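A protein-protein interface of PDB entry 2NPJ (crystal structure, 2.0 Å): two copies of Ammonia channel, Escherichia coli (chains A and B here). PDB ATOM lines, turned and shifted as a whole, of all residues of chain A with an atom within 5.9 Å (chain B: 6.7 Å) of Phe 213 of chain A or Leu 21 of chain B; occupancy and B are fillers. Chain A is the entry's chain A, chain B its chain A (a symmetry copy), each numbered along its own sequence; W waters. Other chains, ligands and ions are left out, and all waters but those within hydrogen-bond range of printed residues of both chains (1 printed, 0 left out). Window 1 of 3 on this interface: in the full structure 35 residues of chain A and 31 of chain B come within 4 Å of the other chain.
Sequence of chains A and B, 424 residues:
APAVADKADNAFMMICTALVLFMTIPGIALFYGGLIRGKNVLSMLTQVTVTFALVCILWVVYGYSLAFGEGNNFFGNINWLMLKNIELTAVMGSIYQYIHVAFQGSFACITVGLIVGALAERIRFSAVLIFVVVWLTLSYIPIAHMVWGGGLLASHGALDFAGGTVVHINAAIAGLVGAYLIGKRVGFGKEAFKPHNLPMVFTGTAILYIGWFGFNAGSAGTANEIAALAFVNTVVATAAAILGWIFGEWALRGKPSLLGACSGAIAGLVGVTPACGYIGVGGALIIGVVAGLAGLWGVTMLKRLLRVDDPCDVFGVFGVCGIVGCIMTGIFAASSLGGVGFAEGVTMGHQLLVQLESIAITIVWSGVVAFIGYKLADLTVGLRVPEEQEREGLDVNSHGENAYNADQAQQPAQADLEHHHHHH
Among the printed residues, merely in contact across the chains: Phe 12 of chain A with Met 14 of chain B (3.7 Å), Tyr 209 of chain A with Leu 21 of chain B (3.97 Å), Tyr 209 of chain A with Phe 52 of chain B (3.3 Å), Ile 210 of chain A with Ala 18 of chain B (3.8 Å), Ile 210 of chain A with Leu 21 of chain B (3.8 Å), Ile 210 of chain A with Phe 22 of chain B (3.5 Å), Ile 210 of chain A with Ile 25 of chain B (3.4 Å), Phe 213 of chain A with Leu 21 of chain B (3.6 Å), Phe 231 of chain A with Met 14 of chain B (3.3 Å), Phe 231 of chain A with Thr 17 of chain B (3.5 Å), Phe 231 of chain A with Ala 18 of chain B (3.8 Å), Phe 231 of chain A with Ala 102 of chain B (3.96 Å) and Val 235 of chain A with Cys 56 of chain B (3.7 Å).
The backbone NH (N) of Gly 27 of chain B is in hydrogen-bond range of the backbone carbonyl oxygen (O) of Phe 22 of chain B (3.1 Å).
The backbone carbonyl oxygen (O) of Phe 52 of chain B sits at hydrogen-bond distance from the side-chain sulfur (SG) of Cys 56 of chain B (3.4 Å).
SG of Cys 109 of chain B is in hydrogen-bond range of SG of Cys 56 of chain B.
Water W1 lies within hydrogen-bond range of the backbone carbonyl oxygen of Val 235 of chain A, the side-chain hydroxyl of Tyr 209 of chain A and the side-chain sulfur of Cys 56 of chain B.
Of the 21 printed residues of chain B, 9 touch a printed residue of chain A.
Printed residues of chain B that touch a printed residue of chain A: Met 14, Thr 17, Ala 18, Leu 21, Phe 22, Ile 25, Phe 52, Cys 56 and Ala 102.
Hydrophobic or aromatic side chains of chain B within 4 Å of the printed part of chain A: Met 14, Leu 21, Phe 22, Phe 52 and Ala 102.
Along chain B the printed residues that touch a printed residue of chain A span positions 14 to 102.
Hydrophobic or aromatic side chains of chain A that line the printed part of chain B: Phe 12, Tyr 209, Ile 210, Phe 213, Phe 231 and Val 235.
Along chain A the printed residues that touch a printed residue of chain B span positions 12 to 235.
Among the printed residues, 13 pairs touch across the chains.
Of chain B, only Leu 21 (3.6 Å) comes within 4 Å of Phe 213 of chain A.
Of the printed residues of chain A, Cys 56 of chain B touches Val 235.
Printed residues of chain A within 4 Å of Phe 22 of chain B: Ile 210.
Of the printed residues of chain B, Val 235 of chain A touches Cys 56 (3.7 Å).
Cys 16 of chain A touches none of the printed residues of chain B.
The nearest residue of chain B that does not touch Phe 213 of chain A is Ala 18 of chain B (4.4 Å).
The nearest printed residue of chain A that does not touch Leu 21 of chain B is Val 235 of chain A (4.2 Å).
The nearest printed residue of chain B that does not touch Ile 210 of chain A is Pro 26 of chain B (5.2 Å).
Positions printed for both chains: 16, 19 and 211.
Of the 13 pairs that touch across the chains among the printed residues, none has its exchanged pair printed and touching as well.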
ATOM      1  N   PHE A  12      36.821 -28.584   9.935  1.00  0.00           N
ATOM      2  CA  PHE A  12      35.406 -28.848   9.750  1.00  0.00           C
ATOM      3  C   PHE A  12      35.030 -30.285  10.139  1.00  0.00           C
ATOM      4  O   PHE A  12      34.037 -30.524  10.850  1.00  0.00           O
ATOM      5  CB  PHE A  12      35.038 -28.612   8.271  1.00  0.00           C
ATOM      6  CG  PHE A  12      33.571 -28.765   7.967  1.00  0.00           C
ATOM      7  CD1 PHE A  12      32.619 -27.963   8.601  1.00  0.00           C
ATOM      8  CD2 PHE A  12      33.141 -29.693   7.019  1.00  0.00           C
ATOM      9  CE1 PHE A  12      31.246 -28.103   8.312  1.00  0.00           C
ATOM     10  CE2 PHE A  12      31.785 -29.834   6.717  1.00  0.00           C
ATOM     11  CZ  PHE A  12      30.835 -29.035   7.369  1.00  0.00           C
ATOM     12  N   CYS A  16      32.715 -31.710  13.016  1.00  0.00           N
ATOM     13  CA  CYS A  16      31.556 -32.532  12.616  1.00  0.00           C
ATOM     14  C   CYS A  16      31.551 -33.877  13.345  1.00  0.00           C
ATOM     15  O   CYS A  16      30.484 -34.375  13.698  1.00  0.00           O
ATOM     16  CB  CYS A  16      31.507 -32.746  11.102  1.00  0.00           C
ATOM     17  SG  CYS A  16      30.948 -31.278  10.187  1.00  0.00           S
ATOM     18  N   LEU A  19      30.323 -33.389  16.799  1.00  0.00           N
ATOM     19  CA  LEU A  19      28.864 -33.208  16.708  1.00  0.00           C
ATOM     20  C   LEU A  19      28.136 -34.553  16.563  1.00  0.00           C
ATOM     21  O   LEU A  19      27.071 -34.749  17.171  1.00  0.00           O
ATOM     22  CB  LEU A  19      28.492 -32.283  15.542  1.00  0.00           C
ATOM     23  CG  LEU A  19      28.693 -30.790  15.866  1.00  0.00           C
ATOM     24  CD1 LEU A  19      28.563 -29.955  14.588  1.00  0.00           C
ATOM     25  CD2 LEU A  19      27.718 -30.290  16.954  1.00  0.00           C
ATOM     26  N   LEU A 208      20.091 -34.233  19.229  1.00  0.00           N
ATOM     27  CA  LEU A 208      20.169 -35.039  18.001  1.00  0.00           C
ATOM     28  C   LEU A 208      20.144 -34.099  16.786  1.00  0.00           C
ATOM     29  O   LEU A 208      20.906 -34.281  15.836  1.00  0.00           O
ATOM     30  CB  LEU A 208      19.001 -36.039  17.923  1.00  0.00           C
ATOM     31  CG  LEU A 208      19.151 -37.313  18.781  1.00  0.00           C
ATOM     32  CD1 LEU A 208      17.815 -38.063  18.938  1.00  0.00           C
ATOM     33  CD2 LEU A 208      20.237 -38.247  18.183  1.00  0.00           C
ATOM     34  N   TYR A 209      19.264 -33.097  16.833  1.00  0.00           N
ATOM     35  CA  TYR A 209      19.122 -32.125  15.745  1.00  0.00           C
ATOM     36  C   TYR A 209      20.418 -31.339  15.492  1.00  0.00           C
ATOM     37  O   TYR A 209      20.913 -31.272  14.360  1.00  0.00           O
ATOM     38  CB  TYR A 209      17.962 -31.172  16.051  1.00  0.00           C
ATOM     39  CG  TYR A 209      17.807 -30.004  15.094  1.00  0.00           C
ATOM     40  CD1 TYR A 209      17.399 -30.203  13.771  1.00  0.00           C
ATOM     41  CD2 TYR A 209      18.052 -28.697  15.519  1.00  0.00           C
ATOM     42  CE1 TYR A 209      17.240 -29.111  12.880  1.00  0.00           C
ATOM     43  CE2 TYR A 209      17.891 -27.603  14.647  1.00  0.00           C
ATOM     44  CZ  TYR A 209      17.487 -27.819  13.334  1.00  0.00           C
ATOM     45  OH  TYR A 209      17.329 -26.736  12.473  1.00  0.00           O
ATOM     46  N   ILE A 210      20.968 -30.745  16.546  1.00  0.00           N
ATOM     47  CA  ILE A 210      22.203 -29.969  16.416  1.00  0.00           C
ATOM     48  C   ILE A 210      23.374 -30.854  15.933  1.00  0.00           C
ATOM     49  O   ILE A 210      24.136 -30.478  15.020  1.00  0.00           O
ATOM     50  CB  ILE A 210      22.529 -29.210  17.749  1.00  0.00           C
ATOM     51  CG1 ILE A 210      21.387 -28.216  18.081  1.00  0.00           C
ATOM     52  CG2 ILE A 210      23.886 -28.468  17.649  1.00  0.00           C
ATOM     53  CD1 ILE A 210      21.095 -27.160  16.973  1.00  0.00           C
ATOM     54  N   GLY A 211      23.506 -32.034  16.534  1.00  0.00           N
ATOM     55  CA  GLY A 211      24.570 -32.966  16.147  1.00  0.00           C
ATOM     56  C   GLY A 211      24.414 -33.428  14.703  1.00  0.00           C
ATOM     57  O   GLY A 211      25.408 -33.703  14.021  1.00  0.00           O
ATOM     58  N   TRP A 212      23.165 -33.488  14.231  1.00  0.00           N
ATOM     59  CA  TRP A 212      22.845 -33.922  12.869  1.00  0.00           C
ATOM     60  C   TRP A 212      23.430 -33.012  11.782  1.00  0.00           C
ATOM     61  O   TRP A 212      23.577 -33.433  10.633  1.00  0.00           O
ATOM     62  CB  TRP A 212      21.330 -34.047  12.689  1.00  0.00           C
ATOM     63  CG  TRP A 212      20.889 -35.268  11.921  1.00  0.00           C
ATOM     64  CD1 TRP A 212      21.169 -35.577  10.612  1.00  0.00           C
ATOM     65  CD2 TRP A 212      20.046 -36.315  12.408  1.00  0.00           C
ATOM     66  NE1 TRP A 212      20.554 -36.762  10.262  1.00  0.00           N
ATOM     67  CE2 TRP A 212      19.851 -37.230  11.344  1.00  0.00           C
ATOM     68  CE3 TRP A 212      19.413 -36.560  13.641  1.00  0.00           C
ATOM     69  CZ2 TRP A 212      19.065 -38.385  11.479  1.00  0.00           C
ATOM     70  CZ3 TRP A 212      18.632 -37.712  13.776  1.00  0.00           C
ATOM     71  CH2 TRP A 212      18.470 -38.608  12.702  1.00  0.00           C
ATOM     72  N   PHE A 213      23.790 -31.779  12.135  1.00  0.00           N
ATOM     73  CA  PHE A 213      24.416 -30.909  11.141  1.00  0.00           C
ATOM     74  C   PHE A 213      25.823 -31.445  10.845  1.00  0.00           C
ATOM     75  O   PHE A 213      26.274 -31.401   9.708  1.00  0.00           O
ATOM     76  CB  PHE A 213      24.392 -29.438  11.576  1.00  0.00           C
ATOM     77  CG  PHE A 213      23.013 -28.849  11.507  1.00  0.00           C
ATOM     78  CD1 PHE A 213      22.456 -28.509  10.273  1.00  0.00           C
ATOM     79  CD2 PHE A 213      22.248 -28.706  12.659  1.00  0.00           C
ATOM     80  CE1 PHE A 213      21.162 -28.000  10.187  1.00  0.00           C
ATOM     81  CE2 PHE A 213      20.945 -28.198  12.588  1.00  0.00           C
ATOM     82  CZ  PHE A 213      20.398 -27.852  11.355  1.00  0.00           C
ATOM     83  N   GLY A 214      26.475 -32.017  11.857  1.00  0.00           N
ATOM     84  CA  GLY A 214      27.800 -32.623  11.660  1.00  0.00           C
ATOM     85  C   GLY A 214      27.623 -33.910  10.855  1.00  0.00           C
ATOM     86  O   GLY A 214      28.416 -34.223   9.959  1.00  0.00           O
ATOM     87  N   PHE A 215      26.555 -34.645  11.177  1.00  0.00           N
ATOM     88  CA  PHE A 215      26.194 -35.924  10.520  1.00  0.00           C
ATOM     89  C   PHE A 215      25.946 -35.709   9.024  1.00  0.00           C
ATOM     90  O   PHE A 215      26.550 -36.384   8.167  1.00  0.00           O
ATOM     91  CB  PHE A 215      24.930 -36.442  11.232  1.00  0.00           C
ATOM     92  CG  PHE A 215      24.483 -37.836  10.862  1.00  0.00           C
ATOM     93  CD1 PHE A 215      23.623 -38.050   9.781  1.00  0.00           C
ATOM     94  CD2 PHE A 215      24.806 -38.920  11.678  1.00  0.00           C
ATOM     95  CE1 PHE A 215      23.154 -39.329   9.474  1.00  0.00           C
ATOM     96  CE2 PHE A 215      24.340 -40.213  11.378  1.00  0.00           C
ATOM     97  CZ  PHE A 215      23.507 -40.418  10.284  1.00  0.00           C
ATOM     98  N   ASN A 216      25.058 -34.767   8.704  1.00  0.00           N
ATOM     99  CA  ASN A 216      24.708 -34.490   7.313  1.00  0.00           C
ATOM    100  C   ASN A 216      25.728 -33.652   6.524  1.00  0.00           C
ATOM    101  O   ASN A 216      26.208 -34.087   5.473  1.00  0.00           O
ATOM    102  CB  ASN A 216      23.304 -33.854   7.215  1.00  0.00           C
ATOM    103  CG  ASN A 216      22.168 -34.879   7.324  1.00  0.00           C
ATOM    104  OD1 ASN A 216      22.399 -36.085   7.386  1.00  0.00           O
ATOM    105  ND2 ASN A 216      20.924 -34.386   7.337  1.00  0.00           N
ATOM    106  N   ALA A 217      26.038 -32.445   7.005  1.00  0.00           N
ATOM    107  CA  ALA A 217      26.998 -31.583   6.303  1.00  0.00           C
ATOM    108  C   ALA A 217      28.414 -32.173   6.274  1.00  0.00           C
ATOM    109  O   ALA A 217      29.124 -32.031   5.277  1.00  0.00           O
ATOM    110  CB  ALA A 217      27.010 -30.169   6.878  1.00  0.00           C
ATOM    111  N   GLY A 218      28.807 -32.859   7.345  1.00  0.00           N
ATOM    112  CA  GLY A 218      30.137 -33.479   7.415  1.00  0.00           C
ATOM    113  C   GLY A 218      30.284 -34.607   6.409  1.00  0.00           C
ATOM    114  O   GLY A 218      31.405 -34.955   6.012  1.00  0.00           O
ATOM    115  N   ALA A 230      23.822 -29.507   1.959  1.00  0.00           N
ATOM    116  CA  ALA A 230      23.347 -30.494   2.928  1.00  0.00           C
ATOM    117  C   ALA A 230      22.904 -29.796   4.215  1.00  0.00           C
ATOM    118  O   ALA A 230      21.918 -30.200   4.836  1.00  0.00           O
ATOM    119  CB  ALA A 230      24.443 -31.516   3.228  1.00  0.00           C
ATOM    120  N   PHE A 231      23.636 -28.753   4.612  1.00  0.00           N
ATOM    121  CA  PHE A 231      23.298 -27.997   5.823  1.00  0.00           C
ATOM    122  C   PHE A 231      21.898 -27.367   5.683  1.00  0.00           C
ATOM    123  O   PHE A 231      21.017 -27.578   6.524  1.00  0.00           O
ATOM    124  CB  PHE A 231      24.338 -26.889   6.091  1.00  0.00           C
ATOM    125  CG  PHE A 231      24.299 -26.352   7.510  1.00  0.00           C
ATOM    126  CD1 PHE A 231      23.240 -25.546   7.943  1.00  0.00           C
ATOM    127  CD2 PHE A 231      25.312 -26.666   8.411  1.00  0.00           C
ATOM    128  CE1 PHE A 231      23.177 -25.073   9.263  1.00  0.00           C
ATOM    129  CE2 PHE A 231      25.271 -26.186   9.734  1.00  0.00           C
ATOM    130  CZ  PHE A 231      24.192 -25.385  10.160  1.00  0.00           C
ATOM    131  N   VAL A 232      21.710 -26.594   4.614  1.00  0.00           N
ATOM    132  CA  VAL A 232      20.435 -25.915   4.344  1.00  0.00           C
ATOM    133  C   VAL A 232      19.291 -26.925   4.198  1.00  0.00           C
ATOM    134  O   VAL A 232      18.207 -26.732   4.764  1.00  0.00           O
ATOM    135  CB  VAL A 232      20.519 -25.008   3.088  1.00  0.00           C
ATOM    136  CG1 VAL A 232      19.131 -24.477   2.695  1.00  0.00           C
ATOM    137  CG2 VAL A 232      21.455 -23.842   3.331  1.00  0.00           C
ATOM    138  N   THR A 234      19.057 -29.774   5.538  1.00  0.00           N
ATOM    139  CA  THR A 234      18.794 -30.354   6.866  1.00  0.00           C
ATOM    140  C   THR A 234      17.832 -29.427   7.623  1.00  0.00           C
ATOM    141  O   THR A 234      16.824 -29.889   8.182  1.00  0.00           O
ATOM    142  CB  THR A 234      20.096 -30.602   7.650  1.00  0.00           C
ATOM    143  OG1 THR A 234      20.899 -31.550   6.930  1.00  0.00           O
ATOM    144  CG2 THR A 234      19.807 -31.174   9.070  1.00  0.00           C
ATOM    145  N   VAL A 235      18.117 -28.124   7.609  1.00  0.00           N
ATOM    146  CA  VAL A 235      17.249 -27.130   8.265  1.00  0.00           C
ATOM    147  C   VAL A 235      15.829 -27.205   7.680  1.00  0.00           C
ATOM    148  O   VAL A 235      14.826 -27.253   8.420  1.00  0.00           O
ATOM    149  CB  VAL A 235      17.778 -25.663   8.061  1.00  0.00           C
ATOM    150  CG1 VAL A 235      16.765 -24.633   8.590  1.00  0.00           C
ATOM    151  CG2 VAL A 235      19.161 -25.449   8.719  1.00  0.00           C
ATOM    152  N   MET B  14      29.423 -22.409   9.039  1.00  0.00           N
ATOM    153  CA  MET B  14      28.455 -23.507   9.172  1.00  0.00           C
ATOM    154  C   MET B  14      28.424 -23.919  10.655  1.00  0.00           C
ATOM    155  O   MET B  14      27.352 -24.147  11.207  1.00  0.00           O
ATOM    156  CB  MET B  14      28.810 -24.706   8.291  1.00  0.00           C
ATOM    157  CG  MET B  14      28.389 -24.510   6.835  1.00  0.00           C
ATOM    158  SD  MET B  14      28.634 -25.979   5.815  1.00  0.00           S
ATOM    159  CE  MET B  14      30.407 -25.861   5.526  1.00  0.00           C
ATOM    160  N   CYS B  16      29.200 -21.967  13.235  1.00  0.00           N
ATOM    161  CA  CYS B  16      28.552 -20.844  13.941  1.00  0.00           C
ATOM    162  C   CYS B  16      27.031 -20.892  13.782  1.00  0.00           C
ATOM    163  O   CYS B  16      26.309 -20.558  14.718  1.00  0.00           O
ATOM    164  CB  CYS B  16      29.094 -19.491  13.474  1.00  0.00           C
ATOM    165  SG  CYS B  16      30.749 -19.118  14.128  1.00  0.00           S
ATOM    166  N   THR B  17      26.545 -21.306  12.605  1.00  0.00           N
ATOM    167  CA  THR B  17      25.103 -21.399  12.353  1.00  0.00           C
ATOM    168  C   THR B  17      24.484 -22.476  13.257  1.00  0.00           C
ATOM    169  O   THR B  17      23.417 -22.258  13.842  1.00  0.00           O
ATOM    170  CB  THR B  17      24.784 -21.730  10.878  1.00  0.00           C
ATOM    171  OG1 THR B  17      25.316 -20.703  10.035  1.00  0.00           O
ATOM    172  CG2 THR B  17      23.275 -21.821  10.655  1.00  0.00           C
ATOM    173  N   ALA B  18      25.152 -23.628  13.362  1.00  0.00           N
ATOM    174  CA  ALA B  18      24.663 -24.717  14.220  1.00  0.00           C
ATOM    175  C   ALA B  18      24.629 -24.214  15.675  1.00  0.00           C
ATOM    176  O   ALA B  18      23.691 -24.510  16.424  1.00  0.00           O
ATOM    177  CB  ALA B  18      25.551 -25.979  14.086  1.00  0.00           C
ATOM    178  N   LEU B  19      25.644 -23.447  16.066  1.00  0.00           N
ATOM    179  CA  LEU B  19      25.683 -22.870  17.421  1.00  0.00           C
ATOM    180  C   LEU B  19      24.505 -21.914  17.661  1.00  0.00           C
ATOM    181  O   LEU B  19      23.921 -21.913  18.757  1.00  0.00           O
ATOM    182  CB  LEU B  19      27.009 -22.142  17.675  1.00  0.00           C
ATOM    183  CG  LEU B  19      28.170 -23.098  18.010  1.00  0.00           C
ATOM    184  CD1 LEU B  19      29.498 -22.336  17.986  1.00  0.00           C
ATOM    185  CD2 LEU B  19      27.967 -23.813  19.365  1.00  0.00           C
ATOM    186  N   VAL B  20      24.150 -21.099  16.663  1.00  0.00           N
ATOM    187  CA  VAL B  20      22.995 -20.176  16.835  1.00  0.00           C
ATOM    188  C   VAL B  20      21.694 -20.987  16.883  1.00  0.00           C
ATOM    189  O   VAL B  20      20.777 -20.671  17.660  1.00  0.00           O
ATOM    190  CB  VAL B  20      22.908 -19.080  15.748  1.00  0.00           C
ATOM    191  CG1 VAL B  20      21.671 -18.168  15.989  1.00  0.00           C
ATOM    192  CG2 VAL B  20      24.189 -18.226  15.733  1.00  0.00           C
ATOM    193  N   LEU B  21      21.596 -22.028  16.055  1.00  0.00           N
ATOM    194  CA  LEU B  21      20.390 -22.871  16.074  1.00  0.00           C
ATOM    195  C   LEU B  21      20.225 -23.519  17.471  1.00  0.00           C
ATOM    196  O   LEU B  21      19.108 -23.650  17.983  1.00  0.00           O
ATOM    197  CB  LEU B  21      20.436 -23.944  14.976  1.00  0.00           C
ATOM    198  CG  LEU B  21      20.294 -23.380  13.545  1.00  0.00           C
ATOM    199  CD1 LEU B  21      20.588 -24.464  12.521  1.00  0.00           C
ATOM    200  CD2 LEU B  21      18.893 -22.796  13.320  1.00  0.00           C
ATOM    201  N   PHE B  22      21.359 -23.888  18.067  1.00  0.00           N
ATOM    202  CA  PHE B  22      21.462 -24.497  19.417  1.00  0.00           C
ATOM    203  C   PHE B  22      20.893 -23.533  20.478  1.00  0.00           C
ATOM    204  O   PHE B  22      20.341 -23.969  21.495  1.00  0.00           O
ATOM    205  CB  PHE B  22      22.953 -24.771  19.669  1.00  0.00           C
ATOM    206  CG  PHE B  22      23.275 -25.608  20.894  1.00  0.00           C
ATOM    207  CD1 PHE B  22      22.480 -26.673  21.289  1.00  0.00           C
ATOM    208  CD2 PHE B  22      24.471 -25.362  21.593  1.00  0.00           C
ATOM    209  CE1 PHE B  22      22.838 -27.476  22.388  1.00  0.00           C
ATOM    210  CE2 PHE B  22      24.839 -26.155  22.695  1.00  0.00           C
ATOM    211  CZ  PHE B  22      24.027 -27.212  23.085  1.00  0.00           C
ATOM    212  N   MET B  23      21.005 -22.227  20.229  1.00  0.00           N
ATOM    213  CA  MET B  23      20.452 -21.213  21.150  1.00  0.00           C
ATOM    214  C   MET B  23      18.930 -21.326  21.274  1.00  0.00           C
ATOM    215  O   MET B  23      18.364 -21.062  22.338  1.00  0.00           O
ATOM    216  CB  MET B  23      20.797 -19.802  20.671  1.00  0.00           C
ATOM    217  CG  MET B  23      22.285 -19.490  20.765  1.00  0.00           C
ATOM    218  SD  MET B  23      22.677 -17.879  20.046  1.00  0.00           S
ATOM    219  CE  MET B  23      21.994 -16.795  21.306  1.00  0.00           C
ATOM    220  N   THR B  24      18.257 -21.684  20.184  1.00  0.00           N
ATOM    221  CA  THR B  24      16.795 -21.838  20.226  1.00  0.00           C
ATOM    222  C   THR B  24      16.439 -23.273  20.619  1.00  0.00           C
ATOM    223  O   THR B  24      15.600 -23.517  21.500  1.00  0.00           O
ATOM    224  CB  THR B  24      16.131 -21.538  18.832  1.00  0.00           C
ATOM    225  OG1 THR B  24      16.471 -20.218  18.391  1.00  0.00           O
ATOM    226  CG2 THR B  24      14.604 -21.680  18.881  1.00  0.00           C
ATOM    227  N   ILE B  25      17.059 -24.225  19.926  1.00  0.00           N
ATOM    228  CA  ILE B  25      16.791 -25.650  20.127  1.00  0.00           C
ATOM    229  C   ILE B  25      18.030 -26.328  20.711  1.00  0.00           C
ATOM    230  O   ILE B  25      18.937 -26.709  19.961  1.00  0.00           O
ATOM    231  CB  ILE B  25      16.366 -26.308  18.756  1.00  0.00           C
ATOM    232  CG1 ILE B  25      15.234 -25.501  18.078  1.00  0.00           C
ATOM    233  CG2 ILE B  25      15.970 -27.787  18.904  1.00  0.00           C
ATOM    234  CD1 ILE B  25      13.845 -25.562  18.802  1.00  0.00           C
ATOM    235  N   PRO B  26      18.067 -26.510  22.049  1.00  0.00           N
ATOM    236  CA  PRO B  26      17.010 -26.245  23.032  1.00  0.00           C
ATOM    237  C   PRO B  26      17.219 -25.050  23.988  1.00  0.00           C
ATOM    238  O   PRO B  26      16.421 -24.880  24.912  1.00  0.00           O
ATOM    239  CB  PRO B  26      17.071 -27.523  23.875  1.00  0.00           C
ATOM    240  CG  PRO B  26      18.623 -27.784  23.967  1.00  0.00           C
ATOM    241  CD  PRO B  26      19.228 -27.160  22.695  1.00  0.00           C
ATOM    242  N   GLY B  27      18.281 -24.265  23.801  1.00  0.00           N
ATOM    243  CA  GLY B  27      18.594 -23.140  24.703  1.00  0.00           C
ATOM    244  C   GLY B  27      17.459 -22.329  25.319  1.00  0.00           C
ATOM    245  O   GLY B  27      17.178 -22.415  26.531  1.00  0.00           O
ATOM    246  N   PHE B  52       9.455 -22.513  15.497  1.00  0.00           N
ATOM    247  CA  PHE B  52      10.827 -22.574  15.005  1.00  0.00           C
ATOM    248  C   PHE B  52      10.763 -23.138  13.578  1.00  0.00           C
ATOM    249  O   PHE B  52      11.352 -22.574  12.652  1.00  0.00           O
ATOM    250  CB  PHE B  52      11.678 -23.479  15.908  1.00  0.00           C
ATOM    251  CG  PHE B  52      13.015 -23.871  15.318  1.00  0.00           C
ATOM    252  CD1 PHE B  52      14.085 -22.985  15.343  1.00  0.00           C
ATOM    253  CD2 PHE B  52      13.212 -25.146  14.777  1.00  0.00           C
ATOM    254  CE1 PHE B  52      15.330 -23.344  14.814  1.00  0.00           C
ATOM    255  CE2 PHE B  52      14.452 -25.515  14.249  1.00  0.00           C
ATOM    256  CZ  PHE B  52      15.510 -24.611  14.263  1.00  0.00           C
ATOM    257  N   CYS B  56      11.777 -21.310   9.944  1.00  0.00           N
ATOM    258  CA  CYS B  56      12.707 -21.927   8.996  1.00  0.00           C
ATOM    259  C   CYS B  56      12.119 -21.973   7.578  1.00  0.00           C
ATOM    260  O   CYS B  56      12.807 -21.643   6.604  1.00  0.00           O
ATOM    261  CB  CYS B  56      13.075 -23.344   9.432  1.00  0.00           C
ATOM    262  SG  CYS B  56      14.142 -23.394  10.873  1.00  0.00           S
ATOM    263  N   ALA B 102      21.572 -19.799   5.659  1.00  0.00           N
ATOM    264  CA  ALA B 102      21.358 -20.542   6.917  1.00  0.00           C
ATOM    265  C   ALA B 102      21.721 -19.717   8.149  1.00  0.00           C
ATOM    266  O   ALA B 102      20.975 -19.729   9.138  1.00  0.00           O
ATOM    267  CB  ALA B 102      22.106 -21.896   6.925  1.00  0.00           C
ATOM    268  N   GLY B 105      19.113 -17.033   8.703  1.00  0.00           N
ATOM    269  CA  GLY B 105      17.877 -17.686   9.134  1.00  0.00           C
ATOM    270  C   GLY B 105      17.898 -18.035  10.616  1.00  0.00           C
ATOM    271  O   GLY B 105      16.869 -17.933  11.302  1.00  0.00           O
ATOM    272  N   SER B 106      19.067 -18.443  11.115  1.00  0.00           N
ATOM    273  CA  SER B 106      19.206 -18.822  12.530  1.00  0.00           C
ATOM    274  C   SER B 106      18.938 -17.649  13.483  1.00  0.00           C
ATOM    275  O   SER B 106      18.444 -17.850  14.597  1.00  0.00           O
ATOM    276  CB  SER B 106      20.555 -19.518  12.799  1.00  0.00           C
ATOM    277  OG  SER B 106      21.657 -18.629  12.689  1.00  0.00           O
ATOM    278  N   PHE B 107      19.245 -16.435  13.030  1.00  0.00           N
ATOM    279  CA  PHE B 107      19.002 -15.212  13.805  1.00  0.00           C
ATOM    280  C   PHE B 107      17.499 -14.929  13.880  1.00  0.00           C
ATOM    281  O   PHE B 107      16.984 -14.494  14.919  1.00  0.00           O
ATOM    282  CB  PHE B 107      19.758 -14.017  13.194  1.00  0.00           C
ATOM    283  CG  PHE B 107      21.175 -13.931  13.652  1.00  0.00           C
ATOM    284  CD1 PHE B 107      22.099 -14.912  13.280  1.00  0.00           C
ATOM    285  CD2 PHE B 107      21.582 -12.903  14.492  1.00  0.00           C
ATOM    286  CE1 PHE B 107      23.420 -14.857  13.726  1.00  0.00           C
ATOM    287  CE2 PHE B 107      22.908 -12.835  14.945  1.00  0.00           C
ATOM    288  CZ  PHE B 107      23.827 -13.812  14.567  1.00  0.00           C
ATOM    289  N   CYS B 109      15.243 -17.206  13.805  1.00  0.00           N
ATOM    290  CA  CYS B 109      14.755 -18.250  14.710  1.00  0.00           C
ATOM    291  C   CYS B 109      14.881 -17.892  16.195  1.00  0.00           C
ATOM    292  O   CYS B 109      13.921 -18.054  16.957  1.00  0.00           O
ATOM    293  CB  CYS B 109      15.478 -19.580  14.423  1.00  0.00           C
ATOM    294  SG  CYS B 109      14.918 -20.351  12.886  1.00  0.00           S
ATOM    295  N   GLY B 211      26.188 -21.090  22.587  1.00  0.00           N
ATOM    296  CA  GLY B 211      25.687 -20.811  21.237  1.00  0.00           C
ATOM    297  C   GLY B 211      25.968 -19.372  20.820  1.00  0.00           C
ATOM    298  O   GLY B 211      26.170 -19.092  19.632  1.00  0.00           O
HETATM  299  O   HOH W   1      15.031 -26.788  11.055  1.00  0.00           O
